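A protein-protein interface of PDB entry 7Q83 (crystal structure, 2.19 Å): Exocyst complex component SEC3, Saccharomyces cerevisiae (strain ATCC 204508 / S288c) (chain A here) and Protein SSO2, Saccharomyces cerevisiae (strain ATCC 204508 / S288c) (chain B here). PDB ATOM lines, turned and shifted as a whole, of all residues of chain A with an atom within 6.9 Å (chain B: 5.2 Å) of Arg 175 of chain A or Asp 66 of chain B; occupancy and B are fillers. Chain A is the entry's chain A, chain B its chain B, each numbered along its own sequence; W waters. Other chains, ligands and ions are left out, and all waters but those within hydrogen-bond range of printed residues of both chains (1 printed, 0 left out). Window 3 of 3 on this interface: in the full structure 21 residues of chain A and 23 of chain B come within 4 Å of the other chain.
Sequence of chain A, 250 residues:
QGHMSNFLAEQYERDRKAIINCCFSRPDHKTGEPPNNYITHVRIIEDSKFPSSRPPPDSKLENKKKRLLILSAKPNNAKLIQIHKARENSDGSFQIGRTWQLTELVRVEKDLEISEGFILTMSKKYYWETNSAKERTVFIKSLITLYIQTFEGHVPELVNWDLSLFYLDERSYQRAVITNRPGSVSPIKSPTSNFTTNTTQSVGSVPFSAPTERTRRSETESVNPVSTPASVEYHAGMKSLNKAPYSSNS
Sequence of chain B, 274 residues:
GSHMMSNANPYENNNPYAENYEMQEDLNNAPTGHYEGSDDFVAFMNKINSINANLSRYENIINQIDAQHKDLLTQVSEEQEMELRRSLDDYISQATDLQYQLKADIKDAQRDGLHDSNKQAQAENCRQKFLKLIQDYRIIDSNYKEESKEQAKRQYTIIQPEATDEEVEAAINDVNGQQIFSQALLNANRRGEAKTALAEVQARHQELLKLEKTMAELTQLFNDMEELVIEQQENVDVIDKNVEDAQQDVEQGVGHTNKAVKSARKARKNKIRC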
ATOM      1  N   GLY A 153     -29.425  20.509 -10.325  1.00  0.00           N
ATOM      2  CA  GLY A 153     -29.322  19.912  -9.013  1.00  0.00           C
ATOM      3  C   GLY A 153     -28.360  20.574  -8.054  1.00  0.00           C
ATOM      4  O   GLY A 153     -28.159  20.049  -6.954  1.00  0.00           O
ATOM      5  N   HIS A 154     -27.756  21.695  -8.424  1.00  0.00           N
ATOM      6  CA  HIS A 154     -26.877  22.422  -7.524  1.00  0.00           C
ATOM      7  C   HIS A 154     -27.593  23.649  -6.970  1.00  0.00           C
ATOM      8  O   HIS A 154     -28.563  24.145  -7.548  1.00  0.00           O
ATOM      9  CB  HIS A 154     -25.587  22.834  -8.236  1.00  0.00           C
ATOM     10  CG  HIS A 154     -24.688  21.682  -8.562  1.00  0.00           C
ATOM     11  ND1 HIS A 154     -24.839  20.920  -9.699  1.00  0.00           N
ATOM     12  CD2 HIS A 154     -23.632  21.159  -7.895  1.00  0.00           C
ATOM     13  CE1 HIS A 154     -23.912  19.979  -9.722  1.00  0.00           C
ATOM     14  NE2 HIS A 154     -23.167  20.102  -8.639  1.00  0.00           N
ATOM     15  N   VAL A 155     -27.105  24.132  -5.832  1.00  0.00           N
ATOM     16  CA  VAL A 155     -27.724  25.271  -5.158  1.00  0.00           C
ATOM     17  C   VAL A 155     -26.640  26.063  -4.435  1.00  0.00           C
ATOM     18  O   VAL A 155     -25.705  25.467  -3.881  1.00  0.00           O
ATOM     19  CB  VAL A 155     -28.837  24.806  -4.200  1.00  0.00           C
ATOM     20  CG1 VAL A 155     -28.263  24.044  -3.009  1.00  0.00           C
ATOM     21  CG2 VAL A 155     -29.682  25.977  -3.730  1.00  0.00           C
ATOM     22  N   GLU A 170     -33.373  19.380   4.665  1.00  0.00           N
ATOM     23  CA  GLU A 170     -32.014  19.521   5.176  1.00  0.00           C
ATOM     24  C   GLU A 170     -31.020  18.708   4.353  1.00  0.00           C
ATOM     25  O   GLU A 170     -30.037  19.252   3.836  1.00  0.00           O
ATOM     26  CB  GLU A 170     -31.960  19.116   6.651  1.00  0.00           C
ATOM     27  CG  GLU A 170     -30.694  19.572   7.356  1.00  0.00           C
ATOM     28  CD  GLU A 170     -30.386  21.036   7.101  1.00  0.00           C
ATOM     29  OE1 GLU A 170     -31.272  21.886   7.337  1.00  0.00           O
ATOM     30  OE2 GLU A 170     -29.259  21.337   6.659  1.00  0.00           O
ATOM     31  N   ARG A 171     -31.260  17.406   4.205  1.00  0.00           N
ATOM     32  CA  ARG A 171     -30.265  16.575   3.542  1.00  0.00           C
ATOM     33  C   ARG A 171     -30.304  16.682   2.020  1.00  0.00           C
ATOM     34  O   ARG A 171     -29.297  16.378   1.372  1.00  0.00           O
ATOM     35  CB  ARG A 171     -30.403  15.114   3.982  1.00  0.00           C
ATOM     36  CG  ARG A 171     -31.691  14.422   3.615  1.00  0.00           C
ATOM     37  CD  ARG A 171     -32.094  13.494   4.747  1.00  0.00           C
ATOM     38  NE  ARG A 171     -32.488  12.173   4.276  1.00  0.00           N
ATOM     39  CZ  ARG A 171     -33.740  11.773   4.112  1.00  0.00           C
ATOM     40  NH1 ARG A 171     -34.761  12.581   4.352  1.00  0.00           N
ATOM     41  NH2 ARG A 171     -33.976  10.531   3.698  1.00  0.00           N
ATOM     42  N   SER A 172     -31.421  17.116   1.428  1.00  0.00           N
ATOM     43  CA  SER A 172     -31.380  17.430   0.002  1.00  0.00           C
ATOM     44  C   SER A 172     -30.562  18.690  -0.256  1.00  0.00           C
ATOM     45  O   SER A 172     -29.913  18.806  -1.302  1.00  0.00           O
ATOM     46  CB  SER A 172     -32.795  17.579  -0.566  1.00  0.00           C
ATOM     47  OG  SER A 172     -33.276  18.909  -0.464  1.00  0.00           O
ATOM     48  N   TYR A 173     -30.567  19.632   0.690  1.00  0.00           N
ATOM     49  CA  TYR A 173     -29.728  20.818   0.554  1.00  0.00           C
ATOM     50  C   TYR A 173     -28.252  20.469   0.714  1.00  0.00           C
ATOM     51  O   TYR A 173     -27.401  20.999  -0.011  1.00  0.00           O
ATOM     52  CB  TYR A 173     -30.150  21.878   1.573  1.00  0.00           C
ATOM     53  CG  TYR A 173     -29.143  22.992   1.753  1.00  0.00           C
ATOM     54  CD1 TYR A 173     -28.987  23.975   0.785  1.00  0.00           C
ATOM     55  CD2 TYR A 173     -28.343  23.053   2.885  1.00  0.00           C
ATOM     56  CE1 TYR A 173     -28.063  24.995   0.945  1.00  0.00           C
ATOM     57  CE2 TYR A 173     -27.415  24.066   3.054  1.00  0.00           C
ATOM     58  CZ  TYR A 173     -27.280  25.036   2.079  1.00  0.00           C
ATOM     59  OH  TYR A 173     -26.360  26.048   2.242  1.00  0.00           O
ATOM     60  N   GLN A 174     -27.929  19.575   1.652  1.00  0.00           N
ATOM     61  CA  GLN A 174     -26.536  19.186   1.846  1.00  0.00           C
ATOM     62  C   GLN A 174     -25.978  18.461   0.627  1.00  0.00           C
ATOM     63  O   GLN A 174     -24.798  18.624   0.299  1.00  0.00           O
ATOM     64  CB  GLN A 174     -26.407  18.310   3.092  1.00  0.00           C
ATOM     65  CG  GLN A 174     -26.602  19.058   4.404  1.00  0.00           C
ATOM     66  CD  GLN A 174     -25.617  20.200   4.581  1.00  0.00           C
ATOM     67  OE1 GLN A 174     -24.480  20.138   4.109  1.00  0.00           O
ATOM     68  NE2 GLN A 174     -26.050  21.250   5.267  1.00  0.00           N
ATOM     69  N   ARG A 175     -26.810  17.674  -0.062  1.00  0.00           N
ATOM     70  CA  ARG A 175     -26.362  16.991  -1.272  1.00  0.00           C
ATOM     71  C   ARG A 175     -26.173  17.959  -2.433  1.00  0.00           C
ATOM     72  O   ARG A 175     -25.353  17.705  -3.321  1.00  0.00           O
ATOM     73  CB  ARG A 175     -27.365  15.907  -1.669  1.00  0.00           C
ATOM     74  CG  ARG A 175     -27.495  14.752  -0.693  1.00  0.00           C
ATOM     75  CD  ARG A 175     -28.489  13.725  -1.216  1.00  0.00           C
ATOM     76  NE  ARG A 175     -27.895  12.895  -2.259  1.00  0.00           N
ATOM     77  CZ  ARG A 175     -28.180  11.615  -2.456  1.00  0.00           C
ATOM     78  NH1 ARG A 175     -29.077  10.985  -1.720  1.00  0.00           N
ATOM     79  NH2 ARG A 175     -27.546  10.949  -3.417  1.00  0.00           N
ATOM     80  N   ALA A 176     -26.920  19.062  -2.445  1.00  0.00           N
ATOM     81  CA  ALA A 176     -26.978  19.948  -3.598  1.00  0.00           C
ATOM     82  C   ALA A 176     -26.104  21.187  -3.471  1.00  0.00           C
ATOM     83  O   ALA A 176     -25.797  21.812  -4.493  1.00  0.00           O
ATOM     84  CB  ALA A 176     -28.424  20.392  -3.844  1.00  0.00           C
ATOM     85  N   VAL A 177     -25.707  21.566  -2.257  1.00  0.00           N
ATOM     86  CA  VAL A 177     -25.014  22.833  -2.063  1.00  0.00           C
ATOM     87  C   VAL A 177     -23.641  22.783  -2.724  1.00  0.00           C
ATOM     88  O   VAL A 177     -22.953  21.754  -2.707  1.00  0.00           O
ATOM     89  CB  VAL A 177     -24.930  23.170  -0.563  1.00  0.00           C
ATOM     90  CG1 VAL A 177     -23.907  22.290   0.148  1.00  0.00           C
ATOM     91  CG2 VAL A 177     -24.626  24.652  -0.363  1.00  0.00           C
ATOM     92  N   ILE A 178     -23.246  23.903  -3.340  1.00  0.00           N
ATOM     93  CA  ILE A 178     -22.032  23.934  -4.147  1.00  0.00           C
ATOM     94  C   ILE A 178     -20.773  23.801  -3.303  1.00  0.00           C
ATOM     95  O   ILE A 178     -19.713  23.446  -3.832  1.00  0.00           O
ATOM     96  CB  ILE A 178     -21.975  25.223  -4.992  1.00  0.00           C
ATOM     97  CG1 ILE A 178     -22.237  26.449  -4.114  1.00  0.00           C
ATOM     98  CG2 ILE A 178     -22.970  25.150  -6.144  1.00  0.00           C
ATOM     99  CD1 ILE A 178     -21.689  27.745  -4.686  1.00  0.00           C
ATOM    100  N   ASN A 180     -20.261  21.501  -1.323  1.00  0.00           N
ATOM    101  CA  ASN A 180     -20.072  20.061  -1.158  1.00  0.00           C
ATOM    102  C   ASN A 180     -19.819  19.689   0.299  1.00  0.00           C
ATOM    103  O   ASN A 180     -20.543  20.125   1.195  1.00  0.00           O
ATOM    104  CB  ASN A 180     -18.921  19.562  -2.035  1.00  0.00           C
ATOM    105  CG  ASN A 180     -19.255  19.608  -3.512  1.00  0.00           C
ATOM    106  OD1 ASN A 180     -20.394  19.361  -3.911  1.00  0.00           O
ATOM    107  ND2 ASN A 180     -18.262  19.927  -4.334  1.00  0.00           N
ATOM    108  N   ILE B  61     -39.280   4.565  -5.339  1.00  0.00           N
ATOM    109  CA  ILE B  61     -38.583   4.336  -6.601  1.00  0.00           C
ATOM    110  C   ILE B  61     -37.341   5.211  -6.683  1.00  0.00           C
ATOM    111  O   ILE B  61     -36.250   4.744  -7.029  1.00  0.00           O
ATOM    112  CB  ILE B  61     -39.527   4.579  -7.791  1.00  0.00           C
ATOM    113  CG1 ILE B  61     -40.457   3.380  -7.979  1.00  0.00           C
ATOM    114  CG2 ILE B  61     -38.735   4.836  -9.059  1.00  0.00           C
ATOM    115  CD1 ILE B  61     -41.725   3.711  -8.725  1.00  0.00           C
ATOM    116  N   ILE B  62     -37.490   6.498  -6.356  1.00  0.00           N
ATOM    117  CA  ILE B  62     -36.336   7.392  -6.314  1.00  0.00           C
ATOM    118  C   ILE B  62     -35.310   6.881  -5.314  1.00  0.00           C
ATOM    119  O   ILE B  62     -34.099   6.923  -5.565  1.00  0.00           O
ATOM    120  CB  ILE B  62     -36.783   8.827  -5.977  1.00  0.00           C
ATOM    121  CG1 ILE B  62     -37.678   9.396  -7.073  1.00  0.00           C
ATOM    122  CG2 ILE B  62     -35.597   9.739  -5.766  1.00  0.00           C
ATOM    123  CD1 ILE B  62     -38.799  10.234  -6.522  1.00  0.00           C
ATOM    124  N   ASN B  63     -35.777   6.389  -4.164  1.00  0.00           N
ATOM    125  CA  ASN B  63     -34.873   5.836  -3.160  1.00  0.00           C
ATOM    126  C   ASN B  63     -34.105   4.639  -3.709  1.00  0.00           C
ATOM    127  O   ASN B  63     -32.917   4.467  -3.413  1.00  0.00           O
ATOM    128  CB  ASN B  63     -35.668   5.452  -1.909  1.00  0.00           C
ATOM    129  CG  ASN B  63     -34.797   4.856  -0.816  1.00  0.00           C
ATOM    130  OD1 ASN B  63     -33.747   5.401  -0.480  1.00  0.00           O
ATOM    131  ND2 ASN B  63     -35.237   3.735  -0.248  1.00  0.00           N
ATOM    132  N   GLN B  64     -34.765   3.803  -4.515  1.00  0.00           N
ATOM    133  CA  GLN B  64     -34.089   2.639  -5.076  1.00  0.00           C
ATOM    134  C   GLN B  64     -33.144   3.028  -6.201  1.00  0.00           C
ATOM    135  O   GLN B  64     -32.117   2.369  -6.398  1.00  0.00           O
ATOM    136  CB  GLN B  64     -35.110   1.618  -5.577  1.00  0.00           C
ATOM    137  CG  GLN B  64     -36.033   1.081  -4.499  1.00  0.00           C
ATOM    138  CD  GLN B  64     -35.284   0.472  -3.330  1.00  0.00           C
ATOM    139  OE1 GLN B  64     -34.160  -0.008  -3.476  1.00  0.00           O
ATOM    140  NE2 GLN B  64     -35.911   0.481  -2.160  1.00  0.00           N
ATOM    141  N   ILE B  65     -33.481   4.075  -6.957  1.00  0.00           N
ATOM    142  CA  ILE B  65     -32.575   4.572  -7.989  1.00  0.00           C
ATOM    143  C   ILE B  65     -31.286   5.074  -7.352  1.00  0.00           C
ATOM    144  O   ILE B  65     -30.178   4.774  -7.816  1.00  0.00           O
ATOM    145  CB  ILE B  65     -33.258   5.673  -8.821  1.00  0.00           C
ATOM    146  CG1 ILE B  65     -34.271   5.058  -9.793  1.00  0.00           C
ATOM    147  CG2 ILE B  65     -32.219   6.503  -9.569  1.00  0.00           C
ATOM    148  CD1 ILE B  65     -35.037   6.083 -10.609  1.00  0.00           C
ATOM    149  N   ASP B  66     -31.417   5.847  -6.272  1.00  0.00           N
ATOM    150  CA  ASP B  66     -30.243   6.293  -5.534  1.00  0.00           C
ATOM    151  C   ASP B  66     -29.413   5.112  -5.051  1.00  0.00           C
ATOM    152  O   ASP B  66     -28.182   5.124  -5.158  1.00  0.00           O
ATOM    153  CB  ASP B  66     -30.673   7.167  -4.356  1.00  0.00           C
ATOM    154  CG  ASP B  66     -29.498   7.764  -3.615  1.00  0.00           C
ATOM    155  OD1 ASP B  66     -28.638   8.396  -4.267  1.00  0.00           O
ATOM    156  OD2 ASP B  66     -29.435   7.598  -2.379  1.00  0.00           O
ATOM    157  N   ALA B  67     -30.072   4.071  -4.534  1.00  0.00           N
ATOM    158  CA  ALA B  67     -29.348   2.911  -4.022  1.00  0.00           C
ATOM    159  C   ALA B  67     -28.582   2.205  -5.130  1.00  0.00           C
ATOM    160  O   ALA B  67     -27.418   1.832  -4.947  1.00  0.00           O
ATOM    161  CB  ALA B  67     -30.315   1.945  -3.345  1.00  0.00           C
ATOM    162  N   GLN B  68     -29.213   2.017  -6.291  1.00  0.00           N
ATOM    163  CA  GLN B  68     -28.535   1.339  -7.388  1.00  0.00           C
ATOM    164  C   GLN B  68     -27.380   2.169  -7.931  1.00  0.00           C
ATOM    165  O   GLN B  68     -26.384   1.605  -8.400  1.00  0.00           O
ATOM    166  CB  GLN B  68     -29.534   1.001  -8.492  1.00  0.00           C
ATOM    167  CG  GLN B  68     -30.326  -0.270  -8.205  1.00  0.00           C
ATOM    168  CD  GLN B  68     -31.753  -0.194  -8.691  1.00  0.00           C
ATOM    169  OE1 GLN B  68     -32.186  -1.004  -9.510  1.00  0.00           O
ATOM    170  NE2 GLN B  68     -32.498   0.778  -8.184  1.00  0.00           N
ATOM    171  N   HIS B  69     -27.486   3.498  -7.869  1.00  0.00           N
ATOM    172  CA  HIS B  69     -26.339   4.345  -8.181  1.00  0.00           C
ATOM    173  C   HIS B  69     -25.168   4.018  -7.266  1.00  0.00           C
ATOM    174  O   HIS B  69     -24.029   3.869  -7.721  1.00  0.00           O
ATOM    175  CB  HIS B  69     -26.720   5.820  -8.048  1.00  0.00           C
ATOM    176  CG  HIS B  69     -27.586   6.329  -9.159  1.00  0.00           C
ATOM    177  ND1 HIS B  69     -28.366   7.459  -9.031  1.00  0.00           N
ATOM    178  CD2 HIS B  69     -27.796   5.865 -10.412  1.00  0.00           C
ATOM    179  CE1 HIS B  69     -29.018   7.670 -10.161  1.00  0.00           C
ATOM    180  NE2 HIS B  69     -28.690   6.716 -11.015  1.00  0.00           N
ATOM    181  N   LYS B  70     -25.438   3.898  -5.963  1.00  0.00           N
ATOM    182  CA  LYS B  70     -24.385   3.581  -5.005  1.00  0.00           C
ATOM    183  C   LYS B  70     -23.814   2.191  -5.254  1.00  0.00           C
ATOM    184  O   LYS B  70     -22.612   1.964  -5.072  1.00  0.00           O
ATOM    185  CB  LYS B  70     -24.930   3.704  -3.582  1.00  0.00           C
ATOM    186  CG  LYS B  70     -25.318   5.124  -3.206  1.00  0.00           C
ATOM    187  CD  LYS B  70     -25.759   5.230  -1.756  1.00  0.00           C
ATOM    188  CE  LYS B  70     -25.983   6.683  -1.364  1.00  0.00           C
ATOM    189  NZ  LYS B  70     -27.422   6.990  -1.126  1.00  0.00           N
ATOM    190  N   ILE B 139     -31.552  16.014  -7.709  1.00  0.00           N
ATOM    191  CA  ILE B 139     -30.284  16.089  -6.987  1.00  0.00           C
ATOM    192  C   ILE B 139     -29.601  14.725  -6.956  1.00  0.00           C
ATOM    193  O   ILE B 139     -28.374  14.625  -7.083  1.00  0.00           O
ATOM    194  CB  ILE B 139     -30.521  16.647  -5.568  1.00  0.00           C
ATOM    195  CG1 ILE B 139     -30.902  18.131  -5.630  1.00  0.00           C
ATOM    196  CG2 ILE B 139     -29.289  16.465  -4.697  1.00  0.00           C
ATOM    197  CD1 ILE B 139     -31.539  18.665  -4.352  1.00  0.00           C
ATOM    198  N   ILE B 140     -30.381  13.653  -6.798  1.00  0.00           N
ATOM    199  CA  ILE B 140     -29.816  12.306  -6.765  1.00  0.00           C
ATOM    200  C   ILE B 140     -29.124  11.976  -8.082  1.00  0.00           C
ATOM    201  O   ILE B 140     -28.022  11.412  -8.100  1.00  0.00           O
ATOM    202  CB  ILE B 140     -30.915  11.284  -6.424  1.00  0.00           C
ATOM    203  CG1 ILE B 140     -31.223  11.337  -4.928  1.00  0.00           C
ATOM    204  CG2 ILE B 140     -30.514   9.876  -6.852  1.00  0.00           C
ATOM    205  CD1 ILE B 140     -32.381  10.473  -4.516  1.00  0.00           C
ATOM    206  N   ASN B 143     -25.795  14.102  -8.304  1.00  0.00           N
ATOM    207  CA  ASN B 143     -24.690  13.517  -7.552  1.00  0.00           C
ATOM    208  C   ASN B 143     -24.107  12.317  -8.280  1.00  0.00           C
ATOM    209  O   ASN B 143     -22.885  12.137  -8.317  1.00  0.00           O
ATOM    210  CB  ASN B 143     -25.156  13.105  -6.156  1.00  0.00           C
ATOM    211  CG  ASN B 143     -25.404  14.287  -5.245  1.00  0.00           C
ATOM    212  OD1 ASN B 143     -25.968  14.139  -4.159  1.00  0.00           O
ATOM    213  ND2 ASN B 143     -24.990  15.470  -5.682  1.00  0.00           N
HETATM  214  O   HOH W   1     -25.144  11.265  -2.903  1.00  0.00           O
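Printed residues of chain A that touch a printed residue of chain B: Gly 153, Ser 172, Arg 175 and Ala 176. Among the printed residues, 7 pairs touch across the chains.
Of chain B, only Asp 66 (2.9 Å), Ile 139 (3.6 Å), Ile 140 (3.9 Å) and Asn 143 (3.0 Å) come within 4 Å of Arg 175 of chain A. Of the printed residues of chain A, Asp 66 of chain B touches Arg 175 (2.9 Å). Of the printed residues of chain A, Asn 143 of chain B touches Arg 175 (3.0 Å). Of the printed residues of chain B, Ser 172 of chain A touches Ile 139. Printed residues of chain B within 4 Å of Ala 176 of chain A: Ile 139. Of the printed residues of chain A, Ile 140 of chain B touches Arg 175 (3.9 Å). Of the printed residues of chain B, Gly 153 of chain A touches Ile 139 (3.6 Å). The nearest printed residue of chain A that does not touch Asp 66 of chain B is Arg 171 of chain A (8.1 Å).
N of Val 155 of chain A lies within hydrogen-bond range of O of Ala 176 of chain A (3.0 Å). The side-chain carboxylate (OD2) of Asp 66 of chain B is in salt-bridge range of the side-chain amino group (NZ) of Lys 70 of chain B, at 2.4 Å.
Water W1 lies within hydrogen-bond range of NH2 of Arg 175 of chain A (2.5 Å) and OD1 of Asn 143 of chain B (3.2 Å).
NH2 of Arg 175 of chain A lies within salt-bridge range of OD1 of Asp 66 of chain B (2.9 Å). The side-chain amide oxygen (OD1) of Asn 143 of chain B is in hydrogen-bond range of the guanidinium group (NE) of Arg 175 of chain A (3.0 Å).
Among the printed residues, pairs that only touch across the chains: Gly 153 of chain A with Ile 139 of chain B, Ser 172 of chain A with Ile 139 of chain B, Arg 175 of chain A with Ile 139 of chain B, Arg 175 of chain A with Ile 140 of chain B and Ala 176 of chain A with Ile 139 of chain B.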
